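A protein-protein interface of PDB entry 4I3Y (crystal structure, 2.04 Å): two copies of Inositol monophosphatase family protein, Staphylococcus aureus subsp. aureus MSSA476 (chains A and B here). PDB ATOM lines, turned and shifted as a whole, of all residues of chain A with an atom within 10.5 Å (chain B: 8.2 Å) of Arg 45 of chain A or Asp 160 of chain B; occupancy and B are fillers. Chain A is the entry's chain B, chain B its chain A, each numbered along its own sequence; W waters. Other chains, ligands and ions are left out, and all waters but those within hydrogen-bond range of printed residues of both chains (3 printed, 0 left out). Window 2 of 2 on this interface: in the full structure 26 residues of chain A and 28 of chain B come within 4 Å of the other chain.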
ATOM      1  N   THR A  39       0.990 -19.876  19.114  1.00  0.00           N
ATOM      2  CA  THR A  39       1.833 -18.748  18.686  1.00  0.00           C
ATOM      3  C   THR A  39       3.026 -18.543  19.612  1.00  0.00           C
ATOM      4  O   THR A  39       2.881 -18.660  20.826  1.00  0.00           O
ATOM      5  CB  THR A  39       0.946 -17.454  18.646  1.00  0.00           C
ATOM      6  OG1 THR A  39      -0.007 -17.612  17.606  1.00  0.00           O
ATOM      7  CG2 THR A  39       1.749 -16.174  18.337  1.00  0.00           C
ATOM      8  N   GLU A  40       4.197 -18.236  19.074  1.00  0.00           N
ATOM      9  CA  GLU A  40       5.422 -17.917  19.890  1.00  0.00           C
ATOM     10  C   GLU A  40       6.082 -16.708  19.223  1.00  0.00           C
ATOM     11  O   GLU A  40       5.756 -16.400  18.052  1.00  0.00           O
ATOM     12  CB  GLU A  40       6.434 -19.052  19.837  1.00  0.00           C
ATOM     13  CG  GLU A  40       5.992 -20.394  20.442  1.00  0.00           C
ATOM     14  CD  GLU A  40       7.057 -21.478  20.269  1.00  0.00           C
ATOM     15  OE1 GLU A  40       7.304 -22.240  21.235  1.00  0.00           O
ATOM     16  OE2 GLU A  40       7.665 -21.572  19.165  1.00  0.00           O
ATOM     17  N   THR A  41       7.003 -16.035  19.932  1.00  0.00           N
ATOM     18  CA  THR A  41       7.742 -14.966  19.309  1.00  0.00           C
ATOM     19  C   THR A  41       9.166 -15.451  19.099  1.00  0.00           C
ATOM     20  O   THR A  41       9.620 -16.325  19.832  1.00  0.00           O
ATOM     21  CB  THR A  41       7.770 -13.702  20.167  1.00  0.00           C
ATOM     22  OG1 THR A  41       8.357 -14.059  21.400  1.00  0.00           O
ATOM     23  CG2 THR A  41       6.326 -13.130  20.428  1.00  0.00           C
ATOM     24  N   LYS A  42       9.864 -14.882  18.112  1.00  0.00           N
ATOM     25  CA  LYS A  42      11.268 -15.222  17.828  1.00  0.00           C
ATOM     26  C   LYS A  42      12.180 -14.067  18.269  1.00  0.00           C
ATOM     27  O   LYS A  42      12.526 -13.923  19.448  1.00  0.00           O
ATOM     28  CB  LYS A  42      11.434 -15.575  16.353  1.00  0.00           C
ATOM     29  CG  LYS A  42      10.474 -16.667  15.908  1.00  0.00           C
ATOM     30  CD  LYS A  42      10.917 -17.316  14.586  1.00  0.00           C
ATOM     31  CE  LYS A  42      10.520 -16.498  13.366  1.00  0.00           C
ATOM     32  NZ  LYS A  42      11.026 -17.081  12.088  1.00  0.00           N
ATOM     33  N   ARG A  43      12.488 -13.174  17.345  1.00  0.00           N
ATOM     34  CA  ARG A  43      13.405 -12.074  17.631  1.00  0.00           C
ATOM     35  C   ARG A  43      12.939 -11.078  18.724  1.00  0.00           C
ATOM     36  O   ARG A  43      13.723 -10.611  19.520  1.00  0.00           O
ATOM     37  CB  ARG A  43      13.671 -11.339  16.295  1.00  0.00           C
ATOM     38  CG  ARG A  43      15.041 -10.716  16.172  1.00  0.00           C
ATOM     39  CD  ARG A  43      15.102  -9.714  14.996  1.00  0.00           C
ATOM     40  NE  ARG A  43      16.151  -8.707  15.221  1.00  0.00           N
ATOM     41  CZ  ARG A  43      16.459  -7.679  14.414  1.00  0.00           C
ATOM     42  NH1 ARG A  43      15.818  -7.459  13.254  1.00  0.00           N
ATOM     43  NH2 ARG A  43      17.455  -6.880  14.768  1.00  0.00           N
ATOM     44  N   HIS A  44      11.664 -10.710  18.714  1.00  0.00           N
ATOM     45  CA  HIS A  44      11.075  -9.748  19.665  1.00  0.00           C
ATOM     46  C   HIS A  44       9.558  -9.950  19.614  1.00  0.00           C
ATOM     47  O   HIS A  44       9.072 -10.804  18.858  1.00  0.00           O
ATOM     48  CB  HIS A  44      11.409  -8.293  19.230  1.00  0.00           C
ATOM     49  CG  HIS A  44      11.293  -8.082  17.758  1.00  0.00           C
ATOM     50  ND1 HIS A  44      10.077  -7.950  17.123  1.00  0.00           N
ATOM     51  CD2 HIS A  44      12.240  -8.060  16.778  1.00  0.00           C
ATOM     52  CE1 HIS A  44      10.279  -7.790  15.825  1.00  0.00           C
ATOM     53  NE2 HIS A  44      11.580  -7.875  15.586  1.00  0.00           N
ATOM     54  N   ARG A  45       8.809  -9.141  20.354  1.00  0.00           N
ATOM     55  CA  ARG A  45       7.352  -9.309  20.447  1.00  0.00           C
ATOM     56  C   ARG A  45       6.563  -9.230  19.108  1.00  0.00           C
ATOM     57  O   ARG A  45       5.434  -9.759  19.000  1.00  0.00           O
ATOM     58  CB  ARG A  45       6.737  -8.413  21.546  1.00  0.00           C
ATOM     59  CG  ARG A  45       6.837  -6.916  21.306  1.00  0.00           C
ATOM     60  CD  ARG A  45       6.125  -6.067  22.380  1.00  0.00           C
ATOM     61  NE  ARG A  45       4.772  -6.562  22.560  1.00  0.00           N
ATOM     62  CZ  ARG A  45       3.664  -6.000  22.064  1.00  0.00           C
ATOM     63  NH1 ARG A  45       3.699  -4.838  21.441  1.00  0.00           N
ATOM     64  NH2 ARG A  45       2.511  -6.597  22.259  1.00  0.00           N
ATOM     65  N   PHE A  46       7.169  -8.635  18.079  1.00  0.00           N
ATOM     66  CA  PHE A  46       6.455  -8.404  16.811  1.00  0.00           C
ATOM     67  C   PHE A  46       6.774  -9.462  15.788  1.00  0.00           C
ATOM     68  O   PHE A  46       6.201  -9.450  14.727  1.00  0.00           O
ATOM     69  CB  PHE A  46       6.808  -7.008  16.271  1.00  0.00           C
ATOM     70  CG  PHE A  46       6.615  -5.929  17.292  1.00  0.00           C
ATOM     71  CD1 PHE A  46       5.333  -5.454  17.599  1.00  0.00           C
ATOM     72  CD2 PHE A  46       7.701  -5.393  17.980  1.00  0.00           C
ATOM     73  CE1 PHE A  46       5.131  -4.464  18.572  1.00  0.00           C
ATOM     74  CE2 PHE A  46       7.514  -4.398  18.953  1.00  0.00           C
ATOM     75  CZ  PHE A  46       6.222  -3.938  19.254  1.00  0.00           C
ATOM     76  N   ASP A  47       7.678 -10.384  16.146  1.00  0.00           N
ATOM     77  CA  ASP A  47       8.257 -11.344  15.229  1.00  0.00           C
ATOM     78  C   ASP A  47       7.657 -12.695  15.563  1.00  0.00           C
ATOM     79  O   ASP A  47       8.147 -13.413  16.448  1.00  0.00           O
ATOM     80  CB  ASP A  47       9.794 -11.398  15.363  1.00  0.00           C
ATOM     81  CG  ASP A  47      10.452 -12.265  14.262  1.00  0.00           C
ATOM     82  OD1 ASP A  47       9.814 -12.456  13.199  1.00  0.00           O
ATOM     83  OD2 ASP A  47      11.590 -12.743  14.453  1.00  0.00           O
ATOM     84  N   LEU A  48       6.571 -13.030  14.892  1.00  0.00           N
ATOM     85  CA  LEU A  48       5.795 -14.179  15.326  1.00  0.00           C
ATOM     86  C   LEU A  48       6.058 -15.472  14.535  1.00  0.00           C
ATOM     87  O   LEU A  48       6.429 -15.444  13.365  1.00  0.00           O
ATOM     88  CB  LEU A  48       4.329 -13.842  15.201  1.00  0.00           C
ATOM     89  CG  LEU A  48       3.838 -12.649  16.025  1.00  0.00           C
ATOM     90  CD1 LEU A  48       2.328 -12.493  15.789  1.00  0.00           C
ATOM     91  CD2 LEU A  48       4.143 -12.832  17.516  1.00  0.00           C
ATOM     92  N   VAL A  49       5.794 -16.610  15.160  1.00  0.00           N
ATOM     93  CA  VAL A  49       5.820 -17.914  14.454  1.00  0.00           C
ATOM     94  C   VAL A  49       4.751 -18.794  15.070  1.00  0.00           C
ATOM     95  O   VAL A  49       4.576 -18.776  16.291  1.00  0.00           O
ATOM     96  CB  VAL A  49       7.209 -18.604  14.456  1.00  0.00           C
ATOM     97  CG1 VAL A  49       7.630 -18.972  15.883  1.00  0.00           C
ATOM     98  CG2 VAL A  49       7.167 -19.847  13.555  1.00  0.00           C
ATOM     99  N   THR A  99       2.956 -13.761   8.821  1.00  0.00           N
ATOM    100  CA  THR A  99       2.543 -14.454  10.057  1.00  0.00           C
ATOM    101  C   THR A  99       1.792 -13.461  10.967  1.00  0.00           C
ATOM    102  O   THR A  99       0.833 -13.842  11.630  1.00  0.00           O
ATOM    103  CB  THR A  99       3.741 -15.059  10.794  1.00  0.00           C
ATOM    104  OG1 THR A  99       4.422 -15.951   9.908  1.00  0.00           O
ATOM    105  CG2 THR A  99       3.289 -15.888  12.101  1.00  0.00           C
ATOM    106  N   ALA A 100       2.221 -12.201  10.986  1.00  0.00           N
ATOM    107  CA  ALA A 100       1.535 -11.183  11.780  1.00  0.00           C
ATOM    108  C   ALA A 100       0.106 -11.074  11.307  1.00  0.00           C
ATOM    109  O   ALA A 100      -0.779 -11.073  12.143  1.00  0.00           O
ATOM    110  CB  ALA A 100       2.275  -9.834  11.760  1.00  0.00           C
ATOM    111  N   ASN A 101      -0.137 -11.012   9.987  1.00  0.00           N
ATOM    112  CA  ASN A 101      -1.528 -11.007   9.471  1.00  0.00           C
ATOM    113  C   ASN A 101      -2.286 -12.308   9.793  1.00  0.00           C
ATOM    114  O   ASN A 101      -3.492 -12.282  10.142  1.00  0.00           O
ATOM    115  CB  ASN A 101      -1.607 -10.749   7.959  1.00  0.00           C
ATOM    116  CG  ASN A 101      -1.264  -9.307   7.592  1.00  0.00           C
ATOM    117  OD1 ASN A 101      -1.330  -8.419   8.464  1.00  0.00           O
ATOM    118  ND2 ASN A 101      -0.944  -9.047   6.274  1.00  0.00           N
ATOM    119  N   VAL A 103      -1.940 -14.127  12.429  1.00  0.00           N
ATOM    120  CA  VAL A 103      -2.282 -14.225  13.844  1.00  0.00           C
ATOM    121  C   VAL A 103      -3.278 -13.155  14.184  1.00  0.00           C
ATOM    122  O   VAL A 103      -4.275 -13.454  14.779  1.00  0.00           O
ATOM    123  CB  VAL A 103      -1.079 -14.065  14.793  1.00  0.00           C
ATOM    124  CG1 VAL A 103      -1.540 -13.845  16.238  1.00  0.00           C
ATOM    125  CG2 VAL A 103      -0.209 -15.277  14.716  1.00  0.00           C
ATOM    126  N   LYS A 104      -3.017 -11.916  13.749  1.00  0.00           N
ATOM    127  CA  LYS A 104      -3.874 -10.761  14.120  1.00  0.00           C
ATOM    128  C   LYS A 104      -5.151 -10.694  13.308  1.00  0.00           C
ATOM    129  O   LYS A 104      -6.109 -10.126  13.808  1.00  0.00           O
ATOM    130  CB  LYS A 104      -3.146  -9.409  13.997  1.00  0.00           C
ATOM    131  CG  LYS A 104      -1.798  -9.369  14.741  1.00  0.00           C
ATOM    132  CD  LYS A 104      -2.081  -9.410  16.261  1.00  0.00           C
ATOM    133  CE  LYS A 104      -0.814  -9.339  17.141  1.00  0.00           C
ATOM    134  NZ  LYS A 104      -1.164  -9.286  18.617  1.00  0.00           N
ATOM    135  N   GLN A 105      -5.181 -11.231  12.082  1.00  0.00           N
ATOM    136  CA  GLN A 105      -6.307 -10.987  11.194  1.00  0.00           C
ATOM    137  C   GLN A 105      -6.893 -12.257  10.592  1.00  0.00           C
ATOM    138  O   GLN A 105      -8.031 -12.218  10.130  1.00  0.00           O
ATOM    139  CB  GLN A 105      -5.873 -10.095  10.020  1.00  0.00           C
ATOM    140  CG  GLN A 105      -5.160  -8.795  10.380  1.00  0.00           C
ATOM    141  CD  GLN A 105      -5.242  -7.824   9.208  1.00  0.00           C
ATOM    142  OE1 GLN A 105      -4.224  -7.539   8.560  1.00  0.00           O
ATOM    143  NE2 GLN A 105      -6.443  -7.405   8.852  1.00  0.00           N
ATOM    144  N   GLN A 168       7.246   2.484   8.974  1.00  0.00           N
ATOM    145  CA  GLN A 168       7.808   2.518  10.361  1.00  0.00           C
ATOM    146  C   GLN A 168       9.317   2.272  10.389  1.00  0.00           C
ATOM    147  O   GLN A 168       9.961   2.493  11.443  1.00  0.00           O
ATOM    148  CB  GLN A 168       7.115   1.468  11.247  1.00  0.00           C
ATOM    149  CG  GLN A 168       5.553   1.406  11.081  1.00  0.00           C
ATOM    150  CD  GLN A 168       4.844   0.385  12.004  1.00  0.00           C
ATOM    151  OE1 GLN A 168       4.122  -0.533  11.530  1.00  0.00           O
ATOM    152  NE2 GLN A 168       5.090   0.507  13.298  1.00  0.00           N
ATOM    153  N   SER B 155     -11.331  -8.309  23.337  1.00  0.00           N
ATOM    154  CA  SER B 155     -10.734  -7.064  23.803  1.00  0.00           C
ATOM    155  C   SER B 155      -9.380  -6.930  23.185  1.00  0.00           C
ATOM    156  O   SER B 155      -8.651  -7.913  23.146  1.00  0.00           O
ATOM    157  CB  SER B 155     -10.514  -7.155  25.305  1.00  0.00           C
ATOM    158  OG  SER B 155     -10.937  -5.939  25.791  1.00  0.00           O
ATOM    159  N   LEU B 156      -9.027  -5.735  22.731  1.00  0.00           N
ATOM    160  CA  LEU B 156      -7.737  -5.529  22.096  1.00  0.00           C
ATOM    161  C   LEU B 156      -7.055  -4.302  22.664  1.00  0.00           C
ATOM    162  O   LEU B 156      -7.497  -3.167  22.390  1.00  0.00           O
ATOM    163  CB  LEU B 156      -7.937  -5.314  20.582  1.00  0.00           C
ATOM    164  CG  LEU B 156      -8.003  -6.374  19.499  1.00  0.00           C
ATOM    165  CD2 LEU B 156      -6.672  -7.099  19.611  1.00  0.00           C
ATOM    166  N   LYS B 157      -5.990  -4.475  23.452  1.00  0.00           N
ATOM    167  CA  LYS B 157      -5.200  -3.304  23.838  1.00  0.00           C
ATOM    168  C   LYS B 157      -4.405  -2.748  22.628  1.00  0.00           C
ATOM    169  O   LYS B 157      -4.012  -3.496  21.731  1.00  0.00           O
ATOM    170  CB  LYS B 157      -4.250  -3.656  24.975  1.00  0.00           C
ATOM    171  CG  LYS B 157      -4.936  -3.840  26.323  1.00  0.00           C
ATOM    172  CD  LYS B 157      -3.933  -3.530  27.405  1.00  0.00           C
ATOM    173  CE  LYS B 157      -3.365  -4.813  27.973  1.00  0.00           C
ATOM    174  NZ  LYS B 157      -4.009  -5.129  29.281  1.00  0.00           N
ATOM    175  N   LEU B 158      -4.128  -1.449  22.595  1.00  0.00           N
ATOM    176  CA  LEU B 158      -3.508  -0.917  21.358  1.00  0.00           C
ATOM    177  C   LEU B 158      -2.158  -1.564  21.004  1.00  0.00           C
ATOM    178  O   LEU B 158      -1.861  -1.795  19.791  1.00  0.00           O
ATOM    179  CB  LEU B 158      -3.397   0.620  21.387  1.00  0.00           C
ATOM    180  CG  LEU B 158      -2.818   1.339  20.153  1.00  0.00           C
ATOM    181  CD1 LEU B 158      -3.736   1.158  18.935  1.00  0.00           C
ATOM    182  CD2 LEU B 158      -2.540   2.800  20.494  1.00  0.00           C
ATOM    183  N   GLU B 159      -1.333  -1.821  22.031  1.00  0.00           N
ATOM    184  CA  GLU B 159      -0.006  -2.484  21.854  1.00  0.00           C
ATOM    185  C   GLU B 159      -0.084  -3.882  21.178  1.00  0.00           C
ATOM    186  O   GLU B 159       0.927  -4.370  20.608  1.00  0.00           O
ATOM    187  CB  GLU B 159       0.736  -2.582  23.199  1.00  0.00           C
ATOM    188  CG  GLU B 159       0.155  -3.683  24.091  1.00  0.00           C
ATOM    189  CD  GLU B 159       0.221  -3.425  25.604  1.00  0.00           C
ATOM    190  OE1 GLU B 159       1.057  -4.052  26.266  1.00  0.00           O
ATOM    191  OE2 GLU B 159      -0.581  -2.638  26.166  1.00  0.00           O
ATOM    192  N   ASP B 160      -1.269  -4.498  21.223  1.00  0.00           N
ATOM    193  CA  ASP B 160      -1.510  -5.804  20.638  1.00  0.00           C
ATOM    194  C   ASP B 160      -2.287  -5.738  19.312  1.00  0.00           C
ATOM    195  O   ASP B 160      -2.724  -6.786  18.781  1.00  0.00           O
ATOM    196  CB  ASP B 160      -2.283  -6.669  21.618  1.00  0.00           C
ATOM    197  CG  ASP B 160      -1.528  -6.856  22.916  1.00  0.00           C
ATOM    198  OD1 ASP B 160      -0.319  -7.100  22.828  1.00  0.00           O
ATOM    199  OD2 ASP B 160      -2.127  -6.710  24.009  1.00  0.00           O
ATOM    200  N   ALA B 161      -2.485  -4.538  18.778  1.00  0.00           N
ATOM    201  CA  ALA B 161      -3.502  -4.424  17.714  1.00  0.00           C
ATOM    202  C   ALA B 161      -2.977  -3.685  16.506  1.00  0.00           C
ATOM    203  O   ALA B 161      -2.118  -2.819  16.652  1.00  0.00           O
ATOM    204  CB  ALA B 161      -4.753  -3.731  18.246  1.00  0.00           C
ATOM    205  N   ILE B 162      -3.507  -4.027  15.325  1.00  0.00           N
ATOM    206  CA  ILE B 162      -3.120  -3.330  14.102  1.00  0.00           C
ATOM    207  C   ILE B 162      -3.968  -2.082  13.993  1.00  0.00           C
ATOM    208  O   ILE B 162      -5.143  -2.133  14.253  1.00  0.00           O
ATOM    209  CB  ILE B 162      -3.301  -4.229  12.833  1.00  0.00           C
ATOM    210  CG1 ILE B 162      -2.292  -5.389  12.894  1.00  0.00           C
ATOM    211  CG2 ILE B 162      -3.191  -3.413  11.547  1.00  0.00           C
ATOM    212  CD1 ILE B 162      -2.559  -6.476  11.860  1.00  0.00           C
ATOM    213  N   ILE B 163      -3.387  -0.948  13.639  1.00  0.00           N
ATOM    214  CA  ILE B 163      -4.280   0.190  13.383  1.00  0.00           C
ATOM    215  C   ILE B 163      -4.180   0.696  11.991  1.00  0.00           C
ATOM    216  O   ILE B 163      -3.198   0.425  11.291  1.00  0.00           O
ATOM    217  CB  ILE B 163      -4.092   1.390  14.317  1.00  0.00           C
ATOM    218  CG1 ILE B 163      -2.665   1.907  14.323  1.00  0.00           C
ATOM    219  CG2 ILE B 163      -4.573   1.045  15.710  1.00  0.00           C
ATOM    220  CD1 ILE B 163      -2.704   3.195  15.150  1.00  0.00           C
ATOM    221  N   ASP B 180       4.387   3.732  17.068  1.00  0.00           N
ATOM    222  CA  ASP B 180       5.041   3.190  18.281  1.00  0.00           C
ATOM    223  C   ASP B 180       4.088   2.496  19.269  1.00  0.00           C
ATOM    224  O   ASP B 180       4.470   1.512  19.879  1.00  0.00           O
ATOM    225  CB  ASP B 180       5.803   4.277  19.064  1.00  0.00           C
ATOM    226  CG  ASP B 180       6.881   4.968  18.237  1.00  0.00           C
ATOM    227  OD1 ASP B 180       7.333   4.386  17.226  1.00  0.00           O
ATOM    228  OD2 ASP B 180       7.249   6.122  18.586  1.00  0.00           O
ATOM    229  N   ALA B 181       2.879   3.019  19.452  1.00  0.00           N
ATOM    230  CA  ALA B 181       1.974   2.478  20.458  1.00  0.00           C
ATOM    231  C   ALA B 181       1.127   1.289  19.987  1.00  0.00           C
ATOM    232  O   ALA B 181       0.508   0.655  20.805  1.00  0.00           O
ATOM    233  CB  ALA B 181       1.060   3.561  20.966  1.00  0.00           C
ATOM    234  N   SER B 182       1.112   0.984  18.684  1.00  0.00           N
ATOM    235  CA  SER B 182       0.278  -0.146  18.170  1.00  0.00           C
ATOM    236  C   SER B 182       1.165  -1.337  17.823  1.00  0.00           C
ATOM    237  O   SER B 182       2.405  -1.229  17.846  1.00  0.00           O
ATOM    238  CB  SER B 182      -0.520   0.284  16.957  1.00  0.00           C
ATOM    239  OG  SER B 182       0.350   0.973  16.108  1.00  0.00           O
ATOM    240  N   PHE B 183       0.543  -2.465  17.503  1.00  0.00           N
ATOM    241  CA  PHE B 183       1.337  -3.663  17.207  1.00  0.00           C
ATOM    242  C   PHE B 183       1.944  -3.488  15.804  1.00  0.00           C
ATOM    243  O   PHE B 183       3.155  -3.735  15.601  1.00  0.00           O
ATOM    244  CB  PHE B 183       0.481  -4.945  17.320  1.00  0.00           C
ATOM    245  CG  PHE B 183       1.226  -6.190  16.993  1.00  0.00           C
ATOM    246  CD1 PHE B 183       1.850  -6.932  18.014  1.00  0.00           C
ATOM    247  CD2 PHE B 183       1.334  -6.613  15.657  1.00  0.00           C
ATOM    248  CE1 PHE B 183       2.591  -8.066  17.728  1.00  0.00           C
ATOM    249  CE2 PHE B 183       2.083  -7.744  15.350  1.00  0.00           C
ATOM    250  CZ  PHE B 183       2.696  -8.469  16.381  1.00  0.00           C
ATOM    251  N   SER B 184       1.102  -3.051  14.869  1.00  0.00           N
ATOM    252  CA  SER B 184       1.549  -2.670  13.476  1.00  0.00           C
ATOM    253  C   SER B 184       0.517  -1.749  12.794  1.00  0.00           C
ATOM    254  O   SER B 184      -0.535  -1.411  13.365  1.00  0.00           O
ATOM    255  CB  SER B 184       1.839  -3.912  12.628  1.00  0.00           C
ATOM    256  OG  SER B 184       2.681  -3.682  11.495  1.00  0.00           O
ATOM    257  N   GLY B 201     -12.570  -7.485  14.423  1.00  0.00           N
ATOM    258  CA  GLY B 201     -11.493  -7.656  15.419  1.00  0.00           C
ATOM    259  C   GLY B 201     -10.091  -7.909  14.835  1.00  0.00           C
ATOM    260  O   GLY B 201      -9.167  -8.238  15.586  1.00  0.00           O
ATOM    261  N   GLN B 202      -9.941  -7.733  13.494  1.00  0.00           N
ATOM    262  CA  GLN B 202      -8.643  -7.769  12.743  1.00  0.00           C
ATOM    263  C   GLN B 202      -7.782  -6.485  12.952  1.00  0.00           C
ATOM    264  O   GLN B 202      -6.567  -6.585  13.052  1.00  0.00           O
ATOM    265  CB  GLN B 202      -8.904  -7.932  11.207  1.00  0.00           C
ATOM    266  CG  GLN B 202      -9.782  -9.154  10.904  1.00  0.00           C
ATOM    267  CD  GLN B 202     -10.177  -9.137   9.439  1.00  0.00           C
ATOM    268  OE1 GLN B 202     -10.882  -8.217   9.007  1.00  0.00           O
ATOM    269  NE2 GLN B 202      -9.714 -10.122   8.668  1.00  0.00           N
ATOM    270  N   PHE B 203      -8.416  -5.311  13.047  1.00  0.00           N
ATOM    271  CA  PHE B 203      -7.756  -4.047  13.430  1.00  0.00           C
ATOM    272  C   PHE B 203      -8.306  -3.621  14.802  1.00  0.00           C
ATOM    273  O   PHE B 203      -9.469  -3.900  15.105  1.00  0.00           O
ATOM    274  CB  PHE B 203      -8.133  -2.940  12.405  1.00  0.00           C
ATOM    275  CG  PHE B 203      -7.551  -3.139  11.016  1.00  0.00           C
ATOM    276  CD1 PHE B 203      -6.623  -4.127  10.769  1.00  0.00           C
ATOM    277  CD2 PHE B 203      -7.846  -2.215   9.998  1.00  0.00           C
ATOM    278  CE1 PHE B 203      -6.069  -4.283   9.467  1.00  0.00           C
ATOM    279  CE2 PHE B 203      -7.305  -2.337   8.731  1.00  0.00           C
ATOM    280  CZ  PHE B 203      -6.420  -3.394   8.454  1.00  0.00           C
ATOM    281  N   GLY B 204      -7.459  -2.952  15.604  1.00  0.00           N
ATOM    282  CA  GLY B 204      -7.883  -2.295  16.845  1.00  0.00           C
ATOM    283  C   GLY B 204      -8.707  -1.069  16.594  1.00  0.00           C
ATOM    284  O   GLY B 204      -9.663  -0.819  17.350  1.00  0.00           O
ATOM    285  N   CYS B 253      -8.944  -0.129  23.235  1.00  0.00           N
ATOM    286  CA  CYS B 253      -7.845   0.758  22.750  1.00  0.00           C
ATOM    287  C   CYS B 253      -8.348   2.152  22.322  1.00  0.00           C
ATOM    288  O   CYS B 253      -7.565   3.052  21.946  1.00  0.00           O
ATOM    289  CB  CYS B 253      -7.051   0.084  21.613  1.00  0.00           C
ATOM    290  SG  CYS B 253      -8.022  -0.374  20.151  1.00  0.00           S
HETATM  291  O   HOH W   1       0.599  -8.578  20.819  1.00  0.00           O
HETATM  292  O   HOH W   2       2.450   0.027  14.575  1.00  0.00           O
HETATM  293  O   HOH W   3      -6.211  -8.754  16.012  1.00  0.00           O
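Hydrophobic or aromatic side chains of chain B that line the printed part of chain A: Ile 162, Phe 183 and Phe 203. Among the printed residues, Asp or Glu carboxylates within 4 Å of a Lys or Arg side-chain nitrogen of the other chain: Arg 45 of chain A with Asp 160 of chain B (2.9 Å).
No position is printed for both chains. Of the 12 pairs that touch across the chains among the printed residues, none has its exchanged pair printed and touching as well.
The backbone carbonyl oxygen of Ala 161 of chain B is in hydrogen-bond range of the backbone NH of Phe 183 of chain B, 2.8 Å away. The backbone NH of Glu 159 of chain B lies within hydrogen-bond range of the backbone carbonyl oxygen of Ala 181 of chain B, at 3.3 Å. N of Ile 163 of chain B is in hydrogen-bond range of O of Ser 184 of chain B (2.9 Å). The backbone NH of Phe 46 of chain A lies close to a ring nitrogen (ND1) of His 44 of chain A, 3.1 Å away. The side-chain amide oxygen of Gln 105 of chain A sits close to the side-chain amide oxygen of Asn 101 of chain A (3.0 Å). O of Ile 162 of chain B sits at hydrogen-bond distance from N of Gly 204 of chain B, 2.8 Å away.
Arg 45 of chain A touches three residues of chain B. Asp 160 of chain B touches just these residues of chain A: Arg 45 (2.9 Å) and Lys 104 (3.0 Å). No residue of chain A comes within 4 Å of Lys 157 of chain B. No residue of chain A comes within 4 Å of Ala 161 of chain B. Of the printed residues of chain A, Ile 162 of chain B touches Lys 104 (3.7 Å) and Gln 105 (3.8 Å). Of the printed residues of chain A, Ser 184 of chain B touches Gln 168. Of the printed residues of chain B, Lys 104 of chain A touches Asp 160 (3.0 Å), Ile 162 (3.7 Å), Phe 183 (3.7 Å) and Gln 202 (3.6 Å). Of the printed residues of chain A, Phe 203 of chain B touches Gln 105 (3.2 Å). Of the printed residues of chain A, Gln 202 of chain B touches Lys 104 and Gln 105. Arg 43 of chain A touches none of the printed residues of chain B. Asp 47 of chain A touches none of the printed residues of chain B.
Water W3 bridges the backbone carbonyl oxygen (O) of Lys 104 of chain A (2.6 Å) and the backbone carbonyl oxygen (O) of Gly 201 of chain B (3.0 Å). Water W1 lies within hydrogen-bond range of the side-chain carboxylate of Asp 160 of chain B (2.7 Å), the side-chain amino group of Lys 104 of chain A (2.9 Å) and the guanidinium group of Arg 45 of chain A (3.1 Å). Water W2 lies within hydrogen-bond range of OG of Ser 182 of chain B (2.8 Å), NE2 of Gln 168 of chain A (3.0 Å) and N of Ser 184 of chain B (3.4 Å).
Arg 45 of chain A touches Phe 183 of chain B. Phe 46 of chain A touches Phe 183 of chain B. Ile 162 of chain B touches Lys 104 of chain A (CD1 to CB, 3.7 Å). CE of Lys 104 of chain A touches CE1 of Phe 183 of chain B (3.7 Å). O of Lys 104 of chain A touches CA of Gln 202 of chain B, at 3.6 Å. Ile 162 of chain B touches Gln 105 of chain A. Phe 203 of chain B touches Gln 105 of chain A.
O of Glu 159 of chain B lies within hydrogen-bond range of NH1 of Arg 45 of chain A, at 2.9 Å. The side-chain carboxylate of Asp 160 of chain B is in salt-bridge range of the guanidinium group of Arg 45 of chain A (2.9 Å). OG of Ser 184 of chain B sits at hydrogen-bond distance from OE1 of Gln 168 of chain A. The backbone carbonyl oxygen (O) of Gln 105 of chain A lies within hydrogen-bond range of the side-chain amide nitrogen (NE2) of Gln 202 of chain B. The side-chain amino group (NZ) of Lys 104 of chain A lies within hydrogen-bond range of the backbone carbonyl oxygen (O) of Asp 160 of chain B (3.0 Å).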
